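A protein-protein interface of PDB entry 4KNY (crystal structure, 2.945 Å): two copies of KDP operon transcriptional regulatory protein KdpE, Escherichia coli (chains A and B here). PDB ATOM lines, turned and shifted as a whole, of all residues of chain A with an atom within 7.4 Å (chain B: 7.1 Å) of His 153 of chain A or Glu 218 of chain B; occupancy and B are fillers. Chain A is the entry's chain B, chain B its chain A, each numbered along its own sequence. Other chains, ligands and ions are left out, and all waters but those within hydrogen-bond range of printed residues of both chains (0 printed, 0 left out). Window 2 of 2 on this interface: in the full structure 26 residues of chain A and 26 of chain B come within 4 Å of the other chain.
The guanidinium group (NH2) of Arg 224 of chain B lies within salt-bridge range of the side-chain carboxylate (OE1) of Glu 151 of chain A, 2.8 Å away. The backbone NH of Val 172 of chain B sits close to the backbone carbonyl oxygen of Ala 142 of chain A.
The backbone NH (N) of Ile 216 of chain B lies within hydrogen-bond range of the backbone carbonyl oxygen (O) of Arg 224 of chain B, 2.9 Å away. SD of Met 226 of chain B sits at hydrogen-bond distance from NH2 of Arg 224 of chain B (3.1 Å). The backbone carbonyl oxygen of His 153 of chain A sits at hydrogen-bond distance from the side-chain amino group of Lys 204 of chain A (3.2 Å). OE2 of Glu 218 of chain B is in salt-bridge range of NH1 of Arg 224 of chain B. The backbone carbonyl oxygen (O) of Ile 221 of chain B sits at hydrogen-bond distance from the backbone NH (N) of Gln 175 of chain B (3.1 Å).
CB of Ala 142 of chain A touches CG of Lys 171 of chain B (3.8 Å). Arg 143 of chain A touches Val 172 of chain B (O to CG1, 3.6 Å). NH2 of Arg 143 of chain A touches CD1 of Ile 221 of chain B, at 3.3 Å. Arg 224 of chain B touches Val 144 of chain A (NE to CG2, 3.8 Å). His 153 of chain A touches Glu 218 of chain B. CD of Pro 156 of chain A touches O of Thr 219 of chain B, 3.8 Å away. Pro 156 of chain A touches Ile 221 of chain B (CB to CD1, 3.8 Å).
Printed residues of chain B within 4 Å of Val 144 of chain A: Arg 224 (3.8 Å). His 153 of chain A touches one residue of chain B. Of the printed residues of chain B, Pro 156 of chain A touches Thr 219 (3.8 Å) and Ile 221 (3.8 Å). Glu 158 of chain A touches none of the printed residues of chain B. Of the printed residues of chain A, Lys 171 of chain B touches Ala 142. Of the printed residues of chain A, Val 172 of chain B touches Ala 142 (3.1 Å) and Arg 143 (3.6 Å). Gln 175 of chain B touches none of the printed residues of chain A. Of chain A, only His 153 comes within 4 Å of Glu 218 of chain B. The nearest residue of chain B that does not touch His 153 of chain A is Thr 219 of chain B (4.8 Å). The nearest residue of chain A that does not touch Glu 218 of chain B is Arg 143 of chain A (4.9 Å). The nearest printed residue of chain B that does not touch Glu 151 of chain A is Met 226 of chain B (4.5 Å).
Of the 14 printed residues of chain A, 6 touch a printed residue of chain B. Of the 15 printed residues of chain B, 6 touch a printed residue of chain A. Among the printed residues, Asp or Glu carboxylates within 4 Å of a Lys or Arg side-chain nitrogen of the other chain: Glu 151 of chain A with Arg 224 of chain B (2.8 Å).
No position is printed for both chains. Of the 9 pairs that touch across the chains among the printed residues, none has its exchanged pair printed and touching as well.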
ATOM      1  N   ALA A 142       7.959 -14.853  25.438  1.00  0.00           N
ATOM      2  CA  ALA A 142       8.591 -16.148  25.666  1.00  0.00           C
ATOM      3  C   ALA A 142      10.098 -16.121  25.432  1.00  0.00           C
ATOM      4  O   ALA A 142      10.788 -17.087  25.746  1.00  0.00           O
ATOM      5  CB  ALA A 142       7.939 -17.220  24.799  1.00  0.00           C
ATOM      6  N   ARG A 143      10.598 -15.016  24.882  1.00  0.00           N
ATOM      7  CA  ARG A 143      12.026 -14.844  24.607  1.00  0.00           C
ATOM      8  C   ARG A 143      12.586 -15.975  23.738  1.00  0.00           C
ATOM      9  O   ARG A 143      13.634 -16.546  24.039  1.00  0.00           O
ATOM     10  CB  ARG A 143      12.823 -14.718  25.912  1.00  0.00           C
ATOM     11  CG  ARG A 143      14.166 -14.013  25.763  1.00  0.00           C
ATOM     12  CD  ARG A 143      14.938 -13.986  27.075  1.00  0.00           C
ATOM     13  NE  ARG A 143      16.150 -13.176  26.980  1.00  0.00           N
ATOM     14  CZ  ARG A 143      16.209 -11.886  27.296  1.00  0.00           C
ATOM     15  NH1 ARG A 143      15.122 -11.261  27.729  1.00  0.00           N
ATOM     16  NH2 ARG A 143      17.350 -11.221  27.178  1.00  0.00           N
ATOM     17  N   VAL A 144      11.877 -16.295  22.660  1.00  0.00           N
ATOM     18  CA  VAL A 144      12.282 -17.372  21.763  1.00  0.00           C
ATOM     19  C   VAL A 144      12.169 -16.955  20.298  1.00  0.00           C
ATOM     20  O   VAL A 144      11.141 -16.434  19.870  1.00  0.00           O
ATOM     21  CB  VAL A 144      11.443 -18.645  22.002  1.00  0.00           C
ATOM     22  CG1 VAL A 144      11.765 -19.703  20.960  1.00  0.00           C
ATOM     23  CG2 VAL A 144      11.684 -19.186  23.400  1.00  0.00           C
ATOM     24  N   ILE A 145      13.233 -17.187  19.533  1.00  0.00           N
ATOM     25  CA  ILE A 145      13.257 -16.828  18.118  1.00  0.00           C
ATOM     26  C   ILE A 145      13.332 -18.071  17.234  1.00  0.00           C
ATOM     27  O   ILE A 145      14.092 -18.993  17.517  1.00  0.00           O
ATOM     28  CB  ILE A 145      14.448 -15.893  17.788  1.00  0.00           C
ATOM     29  CG1 ILE A 145      14.217 -14.496  18.367  1.00  0.00           C
ATOM     30  CG2 ILE A 145      14.672 -15.795  16.287  1.00  0.00           C
ATOM     31  CD1 ILE A 145      14.778 -14.307  19.755  1.00  0.00           C
ATOM     32  N   HIS A 146      12.531 -18.092  16.174  1.00  0.00           N
ATOM     33  CA  HIS A 146      12.593 -19.150  15.174  1.00  0.00           C
ATOM     34  C   HIS A 146      13.017 -18.588  13.820  1.00  0.00           C
ATOM     35  O   HIS A 146      12.809 -17.411  13.534  1.00  0.00           O
ATOM     36  CB  HIS A 146      11.236 -19.843  15.038  1.00  0.00           C
ATOM     37  CG  HIS A 146      10.908 -20.766  16.166  1.00  0.00           C
ATOM     38  ND1 HIS A 146      10.839 -20.347  17.481  1.00  0.00           N
ATOM     39  CD2 HIS A 146      10.623 -22.090  16.184  1.00  0.00           C
ATOM     40  CE1 HIS A 146      10.529 -21.370  18.251  1.00  0.00           C
ATOM     41  NE2 HIS A 146      10.392 -22.443  17.489  1.00  0.00           N
ATOM     42  N   GLU A 151      15.171 -23.263  15.539  1.00  0.00           N
ATOM     43  CA  GLU A 151      15.208 -22.196  16.531  1.00  0.00           C
ATOM     44  C   GLU A 151      16.561 -21.492  16.521  1.00  0.00           C
ATOM     45  O   GLU A 151      17.607 -22.139  16.512  1.00  0.00           O
ATOM     46  CB  GLU A 151      14.913 -22.760  17.924  1.00  0.00           C
ATOM     47  CG  GLU A 151      15.028 -21.745  19.052  1.00  0.00           C
ATOM     48  CD  GLU A 151      14.636 -22.318  20.401  1.00  0.00           C
ATOM     49  OE1 GLU A 151      14.951 -21.685  21.431  1.00  0.00           O
ATOM     50  OE2 GLU A 151      14.010 -23.399  20.430  1.00  0.00           O
ATOM     51  N   VAL A 152      16.534 -20.163  16.517  1.00  0.00           N
ATOM     52  CA  VAL A 152      17.754 -19.365  16.533  1.00  0.00           C
ATOM     53  C   VAL A 152      17.999 -18.786  17.923  1.00  0.00           C
ATOM     54  O   VAL A 152      17.119 -18.150  18.501  1.00  0.00           O
ATOM     55  CB  VAL A 152      17.685 -18.217  15.503  1.00  0.00           C
ATOM     56  CG1 VAL A 152      18.771 -17.183  15.767  1.00  0.00           C
ATOM     57  CG2 VAL A 152      17.792 -18.768  14.088  1.00  0.00           C
ATOM     58  N   HIS A 153      19.194 -19.011  18.461  1.00  0.00           N
ATOM     59  CA  HIS A 153      19.534 -18.497  19.782  1.00  0.00           C
ATOM     60  C   HIS A 153      20.224 -17.142  19.709  1.00  0.00           C
ATOM     61  O   HIS A 153      21.175 -16.957  18.950  1.00  0.00           O
ATOM     62  CB  HIS A 153      20.422 -19.485  20.540  1.00  0.00           C
ATOM     63  CG  HIS A 153      20.754 -19.049  21.935  1.00  0.00           C
ATOM     64  ND1 HIS A 153      19.887 -19.219  22.993  1.00  0.00           N
ATOM     65  CD2 HIS A 153      21.854 -18.447  22.443  1.00  0.00           C
ATOM     66  CE1 HIS A 153      20.442 -18.745  24.094  1.00  0.00           C
ATOM     67  NE2 HIS A 153      21.636 -18.270  23.789  1.00  0.00           N
ATOM     68  N   LEU A 154      19.736 -16.199  20.508  1.00  0.00           N
ATOM     69  CA  LEU A 154      20.370 -14.895  20.632  1.00  0.00           C
ATOM     70  C   LEU A 154      20.921 -14.721  22.043  1.00  0.00           C
ATOM     71  O   LEU A 154      20.311 -15.162  23.016  1.00  0.00           O
ATOM     72  CB  LEU A 154      19.375 -13.774  20.330  1.00  0.00           C
ATOM     73  CG  LEU A 154      18.670 -13.769  18.972  1.00  0.00           C
ATOM     74  CD1 LEU A 154      18.047 -12.408  18.716  1.00  0.00           C
ATOM     75  CD2 LEU A 154      19.623 -14.143  17.852  1.00  0.00           C
ATOM     76  N   THR A 155      22.080 -14.081  22.147  1.00  0.00           N
ATOM     77  CA  THR A 155      22.654 -13.741  23.442  1.00  0.00           C
ATOM     78  C   THR A 155      21.824 -12.601  24.031  1.00  0.00           C
ATOM     79  O   THR A 155      21.094 -11.939  23.293  1.00  0.00           O
ATOM     80  CB  THR A 155      24.126 -13.313  23.294  1.00  0.00           C
ATOM     81  OG1 THR A 155      24.192 -11.990  22.751  1.00  0.00           O
ATOM     82  CG2 THR A 155      24.875 -14.277  22.389  1.00  0.00           C
ATOM     83  N   PRO A 156      21.912 -12.377  25.356  1.00  0.00           N
ATOM     84  CA  PRO A 156      21.101 -11.331  25.997  1.00  0.00           C
ATOM     85  C   PRO A 156      21.177  -9.954  25.330  1.00  0.00           C
ATOM     86  O   PRO A 156      20.129  -9.360  25.073  1.00  0.00           O
ATOM     87  CB  PRO A 156      21.663 -11.272  27.428  1.00  0.00           C
ATOM     88  CG  PRO A 156      22.915 -12.111  27.414  1.00  0.00           C
ATOM     89  CD  PRO A 156      22.690 -13.130  26.353  1.00  0.00           C
ATOM     90  N   GLU A 158      22.170  -9.179  22.232  1.00  0.00           N
ATOM     91  CA  GLU A 158      21.580  -9.321  20.905  1.00  0.00           C
ATOM     92  C   GLU A 158      20.057  -9.247  20.982  1.00  0.00           C
ATOM     93  O   GLU A 158      19.408  -8.640  20.129  1.00  0.00           O
ATOM     94  CB  GLU A 158      21.999 -10.650  20.269  1.00  0.00           C
ATOM     95  CG  GLU A 158      23.479 -10.754  19.933  1.00  0.00           C
ATOM     96  CD  GLU A 158      23.875 -12.150  19.480  1.00  0.00           C
ATOM     97  OE1 GLU A 158      22.993 -13.034  19.439  1.00  0.00           O
ATOM     98  OE2 GLU A 158      25.066 -12.365  19.167  1.00  0.00           O
ATOM     99  N   HIS A 200      25.934  -9.638  14.099  1.00  0.00           N
ATOM    100  CA  HIS A 200      25.382 -10.878  14.637  1.00  0.00           C
ATOM    101  C   HIS A 200      23.892 -11.043  14.330  1.00  0.00           C
ATOM    102  O   HIS A 200      23.441 -12.129  13.935  1.00  0.00           O
ATOM    103  CB  HIS A 200      25.681 -11.016  16.131  1.00  0.00           C
ATOM    104  CG  HIS A 200      27.100 -11.417  16.419  1.00  0.00           C
ATOM    105  ND1 HIS A 200      27.822 -10.887  17.465  1.00  0.00           N
ATOM    106  CD2 HIS A 200      27.919 -12.286  15.793  1.00  0.00           C
ATOM    107  CE1 HIS A 200      29.033 -11.418  17.472  1.00  0.00           C
ATOM    108  NE2 HIS A 200      29.120 -12.273  16.466  1.00  0.00           N
ATOM    109  N   LYS A 204      22.696 -13.903  11.688  1.00  0.00           N
ATOM    110  CA  LYS A 204      21.755 -14.845  12.289  1.00  0.00           C
ATOM    111  C   LYS A 204      20.365 -14.814  11.653  1.00  0.00           C
ATOM    112  O   LYS A 204      19.717 -15.854  11.529  1.00  0.00           O
ATOM    113  CB  LYS A 204      21.650 -14.646  13.801  1.00  0.00           C
ATOM    114  CG  LYS A 204      22.704 -15.394  14.589  1.00  0.00           C
ATOM    115  CD  LYS A 204      22.657 -15.030  16.059  1.00  0.00           C
ATOM    116  CE  LYS A 204      23.703 -15.802  16.842  1.00  0.00           C
ATOM    117  NZ  LYS A 204      23.826 -15.302  18.237  1.00  0.00           N
ATOM    118  N   LYS B 171       8.261 -20.937  27.495  1.00  0.00           N
ATOM    119  CA  LYS B 171       8.708 -19.580  27.783  1.00  0.00           C
ATOM    120  C   LYS B 171       9.908 -19.602  28.721  1.00  0.00           C
ATOM    121  O   LYS B 171       9.910 -20.331  29.714  1.00  0.00           O
ATOM    122  CB  LYS B 171       7.571 -18.787  28.429  1.00  0.00           C
ATOM    123  CG  LYS B 171       6.238 -18.918  27.706  1.00  0.00           C
ATOM    124  CD  LYS B 171       5.065 -18.677  28.644  1.00  0.00           C
ATOM    125  CE  LYS B 171       5.004 -17.233  29.110  1.00  0.00           C
ATOM    126  NZ  LYS B 171       4.661 -16.311  27.992  1.00  0.00           N
ATOM    127  N   VAL B 172      10.930 -18.809  28.415  1.00  0.00           N
ATOM    128  CA  VAL B 172      12.060 -18.700  29.330  1.00  0.00           C
ATOM    129  C   VAL B 172      11.709 -17.798  30.513  1.00  0.00           C
ATOM    130  O   VAL B 172      11.072 -16.753  30.361  1.00  0.00           O
ATOM    131  CB  VAL B 172      13.384 -18.250  28.631  1.00  0.00           C
ATOM    132  CG1 VAL B 172      13.260 -18.333  27.124  1.00  0.00           C
ATOM    133  CG2 VAL B 172      13.800 -16.851  29.062  1.00  0.00           C
ATOM    134  N   LEU B 173      12.093 -18.242  31.701  1.00  0.00           N
ATOM    135  CA  LEU B 173      11.917 -17.461  32.909  1.00  0.00           C
ATOM    136  C   LEU B 173      13.279 -16.992  33.392  1.00  0.00           C
ATOM    137  O   LEU B 173      14.256 -17.754  33.378  1.00  0.00           O
ATOM    138  CB  LEU B 173      11.220 -18.288  33.989  1.00  0.00           C
ATOM    139  CG  LEU B 173       9.757 -18.627  33.706  1.00  0.00           C
ATOM    140  CD1 LEU B 173       9.174 -19.498  34.801  1.00  0.00           C
ATOM    141  CD2 LEU B 173       8.952 -17.351  33.556  1.00  0.00           C
ATOM    142  N   GLN B 175      16.104 -15.551  36.128  1.00  0.00           N
ATOM    143  CA  GLN B 175      16.523 -16.042  37.435  1.00  0.00           C
ATOM    144  C   GLN B 175      15.768 -15.322  38.548  1.00  0.00           C
ATOM    145  O   GLN B 175      15.422 -15.924  39.566  1.00  0.00           O
ATOM    146  CB  GLN B 175      18.035 -15.880  37.601  1.00  0.00           C
ATOM    147  CG  GLN B 175      18.840 -16.639  36.556  1.00  0.00           C
ATOM    148  CD  GLN B 175      20.312 -16.277  36.566  1.00  0.00           C
ATOM    149  OE1 GLN B 175      20.766 -15.485  37.391  1.00  0.00           O
ATOM    150  NE2 GLN B 175      21.070 -16.856  35.640  1.00  0.00           N
ATOM    151  N   ARG B 202      17.253 -31.846  36.589  1.00  0.00           N
ATOM    152  CA  ARG B 202      17.873 -32.468  35.423  1.00  0.00           C
ATOM    153  C   ARG B 202      18.352 -33.881  35.735  1.00  0.00           C
ATOM    154  O   ARG B 202      18.170 -34.798  34.936  1.00  0.00           O
ATOM    155  CB  ARG B 202      19.034 -31.616  34.911  1.00  0.00           C
ATOM    156  CG  ARG B 202      18.607 -30.473  34.012  1.00  0.00           C
ATOM    157  CD  ARG B 202      19.689 -29.413  33.905  1.00  0.00           C
ATOM    158  NE  ARG B 202      19.365 -28.425  32.881  1.00  0.00           N
ATOM    159  CZ  ARG B 202      20.031 -27.289  32.702  1.00  0.00           C
ATOM    160  NH1 ARG B 202      21.060 -26.986  33.484  1.00  0.00           N
ATOM    161  NH2 ARG B 202      19.664 -26.451  31.742  1.00  0.00           N
ATOM    162  N   ILE B 216      16.163 -26.475  29.577  1.00  0.00           N
ATOM    163  CA  ILE B 216      17.201 -25.763  28.838  1.00  0.00           C
ATOM    164  C   ILE B 216      17.700 -24.506  29.552  1.00  0.00           C
ATOM    165  O   ILE B 216      16.912 -23.724  30.086  1.00  0.00           O
ATOM    166  CB  ILE B 216      16.701 -25.399  27.413  1.00  0.00           C
ATOM    167  CG1 ILE B 216      16.823 -26.601  26.470  1.00  0.00           C
ATOM    168  CG2 ILE B 216      17.468 -24.217  26.837  1.00  0.00           C
ATOM    169  CD1 ILE B 216      15.776 -27.678  26.676  1.00  0.00           C
ATOM    170  N   THR B 217      19.019 -24.326  29.557  1.00  0.00           N
ATOM    171  CA  THR B 217      19.637 -23.136  30.126  1.00  0.00           C
ATOM    172  C   THR B 217      19.659 -21.988  29.123  1.00  0.00           C
ATOM    173  O   THR B 217      20.217 -22.118  28.034  1.00  0.00           O
ATOM    174  CB  THR B 217      21.088 -23.415  30.559  1.00  0.00           C
ATOM    175  OG1 THR B 217      21.105 -24.438  31.560  1.00  0.00           O
ATOM    176  CG2 THR B 217      21.734 -22.150  31.114  1.00  0.00           C
ATOM    177  N   GLU B 218      19.043 -20.870  29.492  1.00  0.00           N
ATOM    178  CA  GLU B 218      19.150 -19.647  28.708  1.00  0.00           C
ATOM    179  C   GLU B 218      20.229 -18.773  29.331  1.00  0.00           C
ATOM    180  O   GLU B 218      19.958 -17.987  30.238  1.00  0.00           O
ATOM    181  CB  GLU B 218      17.813 -18.908  28.659  1.00  0.00           C
ATOM    182  CG  GLU B 218      16.726 -19.650  27.896  1.00  0.00           C
ATOM    183  CD  GLU B 218      17.061 -19.826  26.425  1.00  0.00           C
ATOM    184  OE1 GLU B 218      17.530 -18.850  25.799  1.00  0.00           O
ATOM    185  OE2 GLU B 218      16.861 -20.941  25.899  1.00  0.00           O
ATOM    186  N   THR B 219      21.452 -18.930  28.831  1.00  0.00           N
ATOM    187  CA  THR B 219      22.643 -18.328  29.426  1.00  0.00           C
ATOM    188  C   THR B 219      22.534 -16.819  29.630  1.00  0.00           C
ATOM    189  O   THR B 219      22.191 -16.079  28.708  1.00  0.00           O
ATOM    190  CB  THR B 219      23.896 -18.634  28.581  1.00  0.00           C
ATOM    191  OG1 THR B 219      23.875 -20.007  28.167  1.00  0.00           O
ATOM    192  CG2 THR B 219      25.158 -18.366  29.382  1.00  0.00           C
ATOM    193  N   GLY B 220      22.823 -16.373  30.849  1.00  0.00           N
ATOM    194  CA  GLY B 220      22.785 -14.961  31.185  1.00  0.00           C
ATOM    195  C   GLY B 220      21.401 -14.470  31.566  1.00  0.00           C
ATOM    196  O   GLY B 220      21.246 -13.359  32.073  1.00  0.00           O
ATOM    197  N   ILE B 221      20.393 -15.304  31.328  1.00  0.00           N
ATOM    198  CA  ILE B 221      19.008 -14.914  31.562  1.00  0.00           C
ATOM    199  C   ILE B 221      18.327 -15.778  32.619  1.00  0.00           C
ATOM    200  O   ILE B 221      17.959 -15.288  33.686  1.00  0.00           O
ATOM    201  CB  ILE B 221      18.182 -14.961  30.259  1.00  0.00           C
ATOM    202  CG1 ILE B 221      18.785 -14.022  29.213  1.00  0.00           C
ATOM    203  CG2 ILE B 221      16.735 -14.588  30.531  1.00  0.00           C
ATOM    204  CD1 ILE B 221      18.945 -12.597  29.695  1.00  0.00           C
ATOM    205  N   GLY B 222      18.157 -17.062  32.319  1.00  0.00           N
ATOM    206  CA  GLY B 222      17.484 -17.967  33.233  1.00  0.00           C
ATOM    207  C   GLY B 222      17.341 -19.369  32.679  1.00  0.00           C
ATOM    208  O   GLY B 222      18.290 -19.924  32.125  1.00  0.00           O
ATOM    209  N   TYR B 223      16.153 -19.950  32.825  1.00  0.00           N
ATOM    210  CA  TYR B 223      15.928 -21.323  32.372  1.00  0.00           C
ATOM    211  C   TYR B 223      14.593 -21.462  31.650  1.00  0.00           C
ATOM    212  O   TYR B 223      13.765 -20.564  31.705  1.00  0.00           O
ATOM    213  CB  TYR B 223      16.001 -22.298  33.549  1.00  0.00           C
ATOM    214  CG  TYR B 223      17.354 -22.342  34.224  1.00  0.00           C
ATOM    215  CD1 TYR B 223      18.333 -23.231  33.804  1.00  0.00           C
ATOM    216  CD2 TYR B 223      17.653 -21.492  35.280  1.00  0.00           C
ATOM    217  CE1 TYR B 223      19.572 -23.274  34.418  1.00  0.00           C
ATOM    218  CE2 TYR B 223      18.888 -21.527  35.899  1.00  0.00           C
ATOM    219  CZ  TYR B 223      19.842 -22.419  35.465  1.00  0.00           C
ATOM    220  OH  TYR B 223      21.073 -22.457  36.079  1.00  0.00           O
ATOM    221  N   ARG B 224      14.384 -22.589  30.976  1.00  0.00           N
ATOM    222  CA  ARG B 224      13.166 -22.785  30.192  1.00  0.00           C
ATOM    223  C   ARG B 224      12.801 -24.254  30.007  1.00  0.00           C
ATOM    224  O   ARG B 224      13.650 -25.071  29.660  1.00  0.00           O
ATOM    225  CB  ARG B 224      13.309 -22.104  28.828  1.00  0.00           C
ATOM    226  CG  ARG B 224      12.432 -22.686  27.730  1.00  0.00           C
ATOM    227  CD  ARG B 224      12.359 -21.749  26.533  1.00  0.00           C
ATOM    228  NE  ARG B 224      12.489 -22.457  25.263  1.00  0.00           N
ATOM    229  CZ  ARG B 224      13.613 -22.518  24.558  1.00  0.00           C
ATOM    230  NH1 ARG B 224      14.708 -21.909  24.995  1.00  0.00           N
ATOM    231  NH2 ARG B 224      13.643 -23.183  23.411  1.00  0.00           N
ATOM    232  N   MET B 226      10.722 -27.229  27.945  1.00  0.00           N
ATOM    233  CA  MET B 226      10.260 -27.468  26.583  1.00  0.00           C
ATOM    234  C   MET B 226       9.415 -28.731  26.473  1.00  0.00           C
ATOM    235  O   MET B 226       9.583 -29.670  27.252  1.00  0.00           O
ATOM    236  CB  MET B 226      11.444 -27.540  25.617  1.00  0.00           C
ATOM    237  CG  MET B 226      12.108 -26.199  25.354  1.00  0.00           C
ATOM    238  SD  MET B 226      13.191 -26.227  23.913  1.00  0.00           S
ATOM    239  CE  MET B 226      12.058 -26.808  22.652  1.00  0.00           C
